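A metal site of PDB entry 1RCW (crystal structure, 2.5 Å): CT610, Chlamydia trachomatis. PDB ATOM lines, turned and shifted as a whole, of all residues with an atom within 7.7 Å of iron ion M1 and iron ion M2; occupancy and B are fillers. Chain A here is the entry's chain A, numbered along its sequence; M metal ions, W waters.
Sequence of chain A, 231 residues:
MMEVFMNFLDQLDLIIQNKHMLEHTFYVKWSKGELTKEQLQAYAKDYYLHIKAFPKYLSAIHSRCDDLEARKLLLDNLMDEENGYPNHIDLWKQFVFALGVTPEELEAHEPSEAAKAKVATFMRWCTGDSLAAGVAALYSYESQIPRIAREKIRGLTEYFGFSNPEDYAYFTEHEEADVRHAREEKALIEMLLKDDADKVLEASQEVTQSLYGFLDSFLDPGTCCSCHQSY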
ATOM      1  N   ILE A  51     -18.975 -15.260  36.194  1.00  0.00           N
ATOM      2  CA  ILE A  51     -19.692 -14.819  35.030  1.00  0.00           C
ATOM      3  C   ILE A  51     -20.839 -13.873  35.438  1.00  0.00           C
ATOM      4  O   ILE A  51     -21.037 -12.870  34.822  1.00  0.00           O
ATOM      5  CB  ILE A  51     -20.227 -16.060  34.271  1.00  0.00           C
ATOM      6  CG1 ILE A  51     -19.062 -16.877  33.677  1.00  0.00           C
ATOM      7  CG2 ILE A  51     -21.174 -15.693  33.124  1.00  0.00           C
ATOM      8  CD1 ILE A  51     -18.185 -16.155  32.694  1.00  0.00           C
ATOM      9  N   PHE A  54     -19.449 -10.570  36.829  1.00  0.00           N
ATOM     10  CA  PHE A  54     -18.638  -9.688  36.016  1.00  0.00           C
ATOM     11  C   PHE A  54     -19.272  -8.310  35.800  1.00  0.00           C
ATOM     12  O   PHE A  54     -18.601  -7.321  36.038  1.00  0.00           O
ATOM     13  CB  PHE A  54     -18.259 -10.315  34.685  1.00  0.00           C
ATOM     14  CG  PHE A  54     -17.023  -9.760  34.162  1.00  0.00           C
ATOM     15  CD1 PHE A  54     -15.812 -10.278  34.543  1.00  0.00           C
ATOM     16  CD2 PHE A  54     -17.041  -8.643  33.366  1.00  0.00           C
ATOM     17  CE1 PHE A  54     -14.631  -9.720  34.080  1.00  0.00           C
ATOM     18  CE2 PHE A  54     -15.864  -8.095  32.916  1.00  0.00           C
ATOM     19  CZ  PHE A  54     -14.669  -8.615  33.282  1.00  0.00           C
ATOM     20  N   LEU A  58     -17.856  -4.096  36.764  1.00  0.00           N
ATOM     21  CA  LEU A  58     -17.869  -2.877  35.924  1.00  0.00           C
ATOM     22  C   LEU A  58     -18.697  -1.722  36.495  1.00  0.00           C
ATOM     23  O   LEU A  58     -18.259  -0.580  36.506  1.00  0.00           O
ATOM     24  CB  LEU A  58     -18.357  -3.240  34.508  1.00  0.00           C
ATOM     25  CG  LEU A  58     -17.380  -4.101  33.693  1.00  0.00           C
ATOM     26  CD1 LEU A  58     -18.038  -4.800  32.539  1.00  0.00           C
ATOM     27  CD2 LEU A  58     -16.282  -3.237  33.151  1.00  0.00           C
ATOM     28  N   ASN A  77     -18.572  -1.373  27.823  1.00  0.00           N
ATOM     29  CA  ASN A  77     -18.290  -2.773  28.212  1.00  0.00           C
ATOM     30  C   ASN A  77     -19.509  -3.442  28.899  1.00  0.00           C
ATOM     31  O   ASN A  77     -19.879  -4.579  28.623  1.00  0.00           O
ATOM     32  CB  ASN A  77     -17.072  -2.853  29.127  1.00  0.00           C
ATOM     33  CG  ASN A  77     -15.709  -2.751  28.362  1.00  0.00           C
ATOM     34  OD1 ASN A  77     -15.608  -2.185  27.234  1.00  0.00           O
ATOM     35  ND2 ASN A  77     -14.657  -3.283  28.988  1.00  0.00           N
ATOM     36  N   ASP A  80     -22.187  -4.535  26.412  1.00  0.00           N
ATOM     37  CA  ASP A  80     -21.757  -5.728  25.723  1.00  0.00           C
ATOM     38  C   ASP A  80     -21.943  -6.959  26.599  1.00  0.00           C
ATOM     39  O   ASP A  80     -22.329  -7.990  26.095  1.00  0.00           O
ATOM     40  CB  ASP A  80     -20.260  -5.683  25.357  1.00  0.00           C
ATOM     41  CG  ASP A  80     -19.926  -4.740  24.199  1.00  0.00           C
ATOM     42  OD1 ASP A  80     -20.840  -4.291  23.452  1.00  0.00           O
ATOM     43  OD2 ASP A  80     -18.717  -4.397  23.961  1.00  0.00           O
ATOM     44  N   GLU A  81     -21.666  -6.866  27.899  1.00  0.00           N
ATOM     45  CA  GLU A  81     -21.766  -8.067  28.757  1.00  0.00           C
ATOM     46  C   GLU A  81     -23.196  -8.455  29.018  1.00  0.00           C
ATOM     47  O   GLU A  81     -23.535  -9.618  29.069  1.00  0.00           O
ATOM     48  CB  GLU A  81     -21.101  -7.876  30.134  1.00  0.00           C
ATOM     49  CG  GLU A  81     -19.650  -7.403  30.119  1.00  0.00           C
ATOM     50  CD  GLU A  81     -18.672  -8.412  29.537  1.00  0.00           C
ATOM     51  OE1 GLU A  81     -17.553  -8.012  29.118  1.00  0.00           O
ATOM     52  OE2 GLU A  81     -19.044  -9.607  29.515  1.00  0.00           O
ATOM     53  N   GLU A  82     -24.047  -7.472  29.218  1.00  0.00           N
ATOM     54  CA  GLU A  82     -25.319  -7.725  29.921  1.00  0.00           C
ATOM     55  C   GLU A  82     -26.595  -7.313  29.161  1.00  0.00           C
ATOM     56  O   GLU A  82     -27.653  -7.844  29.465  1.00  0.00           O
ATOM     57  CB  GLU A  82     -25.282  -7.118  31.341  1.00  0.00           C
ATOM     58  CG  GLU A  82     -26.167  -7.821  32.338  1.00  0.00           C
ATOM     59  CD  GLU A  82     -26.210  -7.181  33.722  1.00  0.00           C
ATOM     60  OE1 GLU A  82     -26.004  -5.946  33.864  1.00  0.00           O
ATOM     61  OE2 GLU A  82     -26.503  -7.902  34.674  1.00  0.00           O
ATOM     62  N   ASN A  87     -27.349 -12.470  26.286  1.00  0.00           N
ATOM     63  CA  ASN A  87     -26.163 -11.767  26.783  1.00  0.00           C
ATOM     64  C   ASN A  87     -25.082 -12.772  27.180  1.00  0.00           C
ATOM     65  O   ASN A  87     -25.267 -13.995  27.042  1.00  0.00           O
ATOM     66  CB  ASN A  87     -26.509 -10.830  27.941  1.00  0.00           C
ATOM     67  CG  ASN A  87     -26.908 -11.571  29.194  1.00  0.00           C
ATOM     68  OD1 ASN A  87     -26.646 -12.765  29.345  1.00  0.00           O
ATOM     69  ND2 ASN A  87     -27.574 -10.880  30.084  1.00  0.00           N
ATOM     70  N   HIS A  88     -23.959 -12.278  27.701  1.00  0.00           N
ATOM     71  CA  HIS A  88     -22.840 -13.175  27.968  1.00  0.00           C
ATOM     72  C   HIS A  88     -23.212 -14.229  29.013  1.00  0.00           C
ATOM     73  O   HIS A  88     -22.855 -15.375  28.867  1.00  0.00           O
ATOM     74  CB  HIS A  88     -21.538 -12.375  28.276  1.00  0.00           C
ATOM     75  CG  HIS A  88     -21.017 -11.663  27.056  1.00  0.00           C
ATOM     76  ND1 HIS A  88     -19.798 -11.042  27.003  1.00  0.00           N
ATOM     77  CD2 HIS A  88     -21.596 -11.477  25.837  1.00  0.00           C
ATOM     78  CE1 HIS A  88     -19.646 -10.479  25.805  1.00  0.00           C
ATOM     79  NE2 HIS A  88     -20.708 -10.750  25.072  1.00  0.00           N
ATOM     80  N   ILE A  89     -24.001 -13.867  30.021  1.00  0.00           N
ATOM     81  CA  ILE A  89     -24.457 -14.856  30.967  1.00  0.00           C
ATOM     82  C   ILE A  89     -25.274 -15.917  30.251  1.00  0.00           C
ATOM     83  O   ILE A  89     -24.994 -17.108  30.364  1.00  0.00           O
ATOM     84  CB  ILE A  89     -25.233 -14.216  32.138  1.00  0.00           C
ATOM     85  CG1 ILE A  89     -24.297 -13.369  33.005  1.00  0.00           C
ATOM     86  CG2 ILE A  89     -25.845 -15.260  33.043  1.00  0.00           C
ATOM     87  CD1 ILE A  89     -25.019 -12.215  33.668  1.00  0.00           C
ATOM     88  N   LEU A  91     -25.128 -16.842  27.247  1.00  0.00           N
ATOM     89  CA  LEU A  91     -24.301 -17.647  26.388  1.00  0.00           C
ATOM     90  C   LEU A  91     -23.529 -18.647  27.219  1.00  0.00           C
ATOM     91  O   LEU A  91     -23.348 -19.813  26.806  1.00  0.00           O
ATOM     92  CB  LEU A  91     -23.341 -16.820  25.555  1.00  0.00           C
ATOM     93  CG  LEU A  91     -23.961 -15.890  24.524  1.00  0.00           C
ATOM     94  CD1 LEU A  91     -22.897 -15.016  23.857  1.00  0.00           C
ATOM     95  CD2 LEU A  91     -24.692 -16.650  23.480  1.00  0.00           C
ATOM     96  N   TYR A 141      -7.708 -10.261  33.463  1.00  0.00           N
ATOM     97  CA  TYR A 141      -8.479 -11.446  33.060  1.00  0.00           C
ATOM     98  C   TYR A 141      -8.906 -11.298  31.588  1.00  0.00           C
ATOM     99  O   TYR A 141      -8.557 -12.092  30.733  1.00  0.00           O
ATOM    100  CB  TYR A 141      -9.706 -11.590  33.989  1.00  0.00           C
ATOM    101  CG  TYR A 141     -10.704 -12.688  33.600  1.00  0.00           C
ATOM    102  CD1 TYR A 141     -10.456 -14.009  33.916  1.00  0.00           C
ATOM    103  CD2 TYR A 141     -11.892 -12.381  32.938  1.00  0.00           C
ATOM    104  CE1 TYR A 141     -11.369 -15.009  33.560  1.00  0.00           C
ATOM    105  CE2 TYR A 141     -12.826 -13.393  32.579  1.00  0.00           C
ATOM    106  CZ  TYR A 141     -12.547 -14.680  32.904  1.00  0.00           C
ATOM    107  OH  TYR A 141     -13.419 -15.677  32.577  1.00  0.00           O
ATOM    108  N   GLU A 142      -9.623 -10.237  31.276  1.00  0.00           N
ATOM    109  CA  GLU A 142     -10.108 -10.048  29.929  1.00  0.00           C
ATOM    110  C   GLU A 142      -8.980 -10.083  28.898  1.00  0.00           C
ATOM    111  O   GLU A 142      -9.170 -10.636  27.825  1.00  0.00           O
ATOM    112  CB  GLU A 142     -11.021  -8.801  29.789  1.00  0.00           C
ATOM    113  CG  GLU A 142     -12.449  -9.161  30.156  1.00  0.00           C
ATOM    114  CD  GLU A 142     -13.484  -8.067  29.984  1.00  0.00           C
ATOM    115  OE1 GLU A 142     -14.520  -8.327  29.327  1.00  0.00           O
ATOM    116  OE2 GLU A 142     -13.292  -6.997  30.556  1.00  0.00           O
ATOM    117  N   ILE A 145      -8.586 -13.606  27.583  1.00  0.00           N
ATOM    118  CA  ILE A 145      -9.683 -14.408  27.035  1.00  0.00           C
ATOM    119  C   ILE A 145      -9.667 -14.624  25.498  1.00  0.00           C
ATOM    120  O   ILE A 145      -9.929 -15.745  25.046  1.00  0.00           O
ATOM    121  CB  ILE A 145     -11.026 -13.868  27.545  1.00  0.00           C
ATOM    122  CG1 ILE A 145     -11.167 -14.117  29.064  1.00  0.00           C
ATOM    123  CG2 ILE A 145     -12.174 -14.509  26.812  1.00  0.00           C
ATOM    124  CD1 ILE A 145     -11.467 -15.597  29.464  1.00  0.00           C
ATOM    125  N   TYR A 170     -20.470 -18.732  23.315  1.00  0.00           N
ATOM    126  CA  TYR A 170     -19.825 -17.858  24.303  1.00  0.00           C
ATOM    127  C   TYR A 170     -18.427 -17.549  23.863  1.00  0.00           C
ATOM    128  O   TYR A 170     -17.977 -16.420  23.997  1.00  0.00           O
ATOM    129  CB  TYR A 170     -19.751 -18.493  25.699  1.00  0.00           C
ATOM    130  CG  TYR A 170     -19.088 -17.609  26.744  1.00  0.00           C
ATOM    131  CD1 TYR A 170     -19.821 -16.650  27.465  1.00  0.00           C
ATOM    132  CD2 TYR A 170     -17.721 -17.706  27.006  1.00  0.00           C
ATOM    133  CE1 TYR A 170     -19.180 -15.806  28.433  1.00  0.00           C
ATOM    134  CE2 TYR A 170     -17.081 -16.882  27.964  1.00  0.00           C
ATOM    135  CZ  TYR A 170     -17.796 -15.950  28.668  1.00  0.00           C
ATOM    136  OH  TYR A 170     -17.128 -15.173  29.596  1.00  0.00           O
ATOM    137  N   GLU A 173     -18.091 -15.604  20.689  1.00  0.00           N
ATOM    138  CA  GLU A 173     -18.310 -14.209  21.039  1.00  0.00           C
ATOM    139  C   GLU A 173     -17.044 -13.560  21.594  1.00  0.00           C
ATOM    140  O   GLU A 173     -16.651 -12.460  21.123  1.00  0.00           O
ATOM    141  CB  GLU A 173     -19.446 -14.065  22.083  1.00  0.00           C
ATOM    142  CG  GLU A 173     -20.674 -13.303  21.579  1.00  0.00           C
ATOM    143  CD  GLU A 173     -20.280 -12.005  20.896  1.00  0.00           C
ATOM    144  OE1 GLU A 173     -19.906 -11.052  21.617  1.00  0.00           O
ATOM    145  OE2 GLU A 173     -20.335 -11.965  19.635  1.00  0.00           O
ATOM    146  N   HIS A 174     -16.414 -14.256  22.546  1.00  0.00           N
ATOM    147  CA  HIS A 174     -15.315 -13.700  23.296  1.00  0.00           C
ATOM    148  C   HIS A 174     -13.969 -13.619  22.537  1.00  0.00           C
ATOM    149  O   HIS A 174     -13.168 -12.709  22.816  1.00  0.00           O
ATOM    150  CB  HIS A 174     -15.199 -14.410  24.636  1.00  0.00           C
ATOM    151  CG  HIS A 174     -16.239 -13.972  25.592  1.00  0.00           C
ATOM    152  ND1 HIS A 174     -17.566 -14.275  25.405  1.00  0.00           N
ATOM    153  CD2 HIS A 174     -16.183 -13.141  26.645  1.00  0.00           C
ATOM    154  CE1 HIS A 174     -18.283 -13.703  26.355  1.00  0.00           C
ATOM    155  NE2 HIS A 174     -17.459 -13.005  27.124  1.00  0.00           N
ATOM    156  N   ALA A 177     -15.020 -10.077  21.085  1.00  0.00           N
ATOM    157  CA  ALA A 177     -15.503  -9.057  22.026  1.00  0.00           C
ATOM    158  C   ALA A 177     -14.408  -8.578  22.957  1.00  0.00           C
ATOM    159  O   ALA A 177     -14.214  -7.366  23.146  1.00  0.00           O
ATOM    160  CB  ALA A 177     -16.661  -9.603  22.839  1.00  0.00           C
ATOM    161  N   ASP A 178     -13.653  -9.521  23.509  1.00  0.00           N
ATOM    162  CA  ASP A 178     -12.687  -9.136  24.496  1.00  0.00           C
ATOM    163  C   ASP A 178     -11.452  -8.489  23.909  1.00  0.00           C
ATOM    164  O   ASP A 178     -10.676  -7.886  24.663  1.00  0.00           O
ATOM    165  CB  ASP A 178     -12.350 -10.295  25.435  1.00  0.00           C
ATOM    166  CG  ASP A 178     -13.440 -10.557  26.446  1.00  0.00           C
ATOM    167  OD1 ASP A 178     -14.510  -9.970  26.312  1.00  0.00           O
ATOM    168  OD2 ASP A 178     -13.330 -11.357  27.397  1.00  0.00           O
ATOM    169  N   VAL A 179     -11.271  -8.563  22.589  1.00  0.00           N
ATOM    170  CA  VAL A 179     -10.169  -7.798  21.962  1.00  0.00           C
ATOM    171  C   VAL A 179     -10.499  -6.320  22.202  1.00  0.00           C
ATOM    172  O   VAL A 179      -9.650  -5.551  22.666  1.00  0.00           O
ATOM    173  CB  VAL A 179      -9.981  -8.076  20.408  1.00  0.00           C
ATOM    174  CG1 VAL A 179      -8.986  -7.142  19.838  1.00  0.00           C
ATOM    175  CG2 VAL A 179      -9.502  -9.458  20.170  1.00  0.00           C
ATOM    176  N   ARG A 180     -11.751  -5.958  21.899  1.00  0.00           N
ATOM    177  CA  ARG A 180     -12.245  -4.609  22.143  1.00  0.00           C
ATOM    178  C   ARG A 180     -12.130  -4.256  23.613  1.00  0.00           C
ATOM    179  O   ARG A 180     -11.618  -3.197  23.969  1.00  0.00           O
ATOM    180  CB  ARG A 180     -13.714  -4.488  21.716  1.00  0.00           C
ATOM    181  CG  ARG A 180     -14.309  -3.104  21.836  1.00  0.00           C
ATOM    182  CD  ARG A 180     -15.707  -2.949  21.163  1.00  0.00           C
ATOM    183  NE  ARG A 180     -16.667  -3.994  21.521  1.00  0.00           N
ATOM    184  CZ  ARG A 180     -16.922  -5.107  20.813  1.00  0.00           C
ATOM    185  NH1 ARG A 180     -16.284  -5.371  19.676  1.00  0.00           N
ATOM    186  NH2 ARG A 180     -17.819  -5.987  21.254  1.00  0.00           N
ATOM    187  N   HIS A 181     -12.605  -5.135  24.480  1.00  0.00           N
ATOM    188  CA  HIS A 181     -12.629  -4.765  25.892  1.00  0.00           C
ATOM    189  C   HIS A 181     -11.236  -4.596  26.470  1.00  0.00           C
ATOM    190  O   HIS A 181     -11.060  -3.748  27.355  1.00  0.00           O
ATOM    191  CB  HIS A 181     -13.417  -5.775  26.730  1.00  0.00           C
ATOM    192  CG  HIS A 181     -14.848  -5.863  26.345  1.00  0.00           C
ATOM    193  ND1 HIS A 181     -15.671  -6.876  26.772  1.00  0.00           N
ATOM    194  CD2 HIS A 181     -15.596  -5.063  25.549  1.00  0.00           C
ATOM    195  CE1 HIS A 181     -16.879  -6.705  26.255  1.00  0.00           C
ATOM    196  NE2 HIS A 181     -16.858  -5.615  25.500  1.00  0.00           N
ATOM    197  N   ALA A 182     -10.269  -5.377  25.996  1.00  0.00           N
ATOM    198  CA  ALA A 182      -8.908  -5.250  26.500  1.00  0.00           C
ATOM    199  C   ALA A 182      -8.356  -3.924  26.100  1.00  0.00           C
ATOM    200  O   ALA A 182      -7.780  -3.223  26.892  1.00  0.00           O
ATOM    201  CB  ALA A 182      -8.028  -6.382  25.995  1.00  0.00           C
ATOM    202  N   GLU A 185     -10.001  -1.218  28.210  1.00  0.00           N
ATOM    203  CA  GLU A 185      -9.507  -1.246  29.574  1.00  0.00           C
ATOM    204  C   GLU A 185      -8.109  -0.672  29.714  1.00  0.00           C
ATOM    205  O   GLU A 185      -7.839   0.042  30.704  1.00  0.00           O
ATOM    206  CB  GLU A 185      -9.581  -2.627  30.138  1.00  0.00           C
ATOM    207  CG  GLU A 185     -11.024  -3.053  30.287  1.00  0.00           C
ATOM    208  CD  GLU A 185     -11.212  -4.535  30.458  1.00  0.00           C
ATOM    209  OE1 GLU A 185     -12.361  -4.863  30.717  1.00  0.00           O
ATOM    210  OE2 GLU A 185     -10.235  -5.316  30.350  1.00  0.00           O
HETATM  211 FE    FE M   1     -18.031 -11.178  28.354  1.00  0.00          FE
HETATM  212 FE    FE M   2     -15.663  -8.963  28.053  1.00  0.00          FE
HETATM  213  O   HOH W   1     -15.592 -11.258  30.161  1.00  0.00           O
HETATM  214  O   HOH W   2     -18.531 -12.596  30.048  1.00  0.00           O
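The backbone carbonyl oxygen (O) of Asp 80 lies within hydrogen-bond range of a ring nitrogen (NE2) of His 88, 3.4 Å away. A ring nitrogen (ND1) of His 174 is in hydrogen-bond range of the backbone carbonyl oxygen of Tyr 170, at 2.6 Å. NE2 of His 181 lies within hydrogen-bond range of OD2 of Asp 80, 2.7 Å away.
The nearest printed residue that does not touch iron ion M1 is Asp 178 (4.2 Å).
Within 4 Å of iron ion M2: Glu 81, Glu 142, Asp 178 and His 181.
OE2 of Glu 81 is bound to iron ion M1 (2.2 Å). ND1 of His 88 is bound to iron ion M1. Water W2 is bound to iron ion M1 (2.3 Å). A ring nitrogen (NE2) of His 174 binds iron ion M1, at 2.3 Å.
OE1 of Glu 142 binds iron ion M2, 1.8 Å away. Iron ion M2 is bound by OD1 of Asp 178, 2.3 Å away. The side-chain carboxylate (OE1) of Glu 81 is bound to iron ion M2 (2.4 Å). A ring nitrogen (ND1) of His 181 binds iron ion M2, 2.4 Å away.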
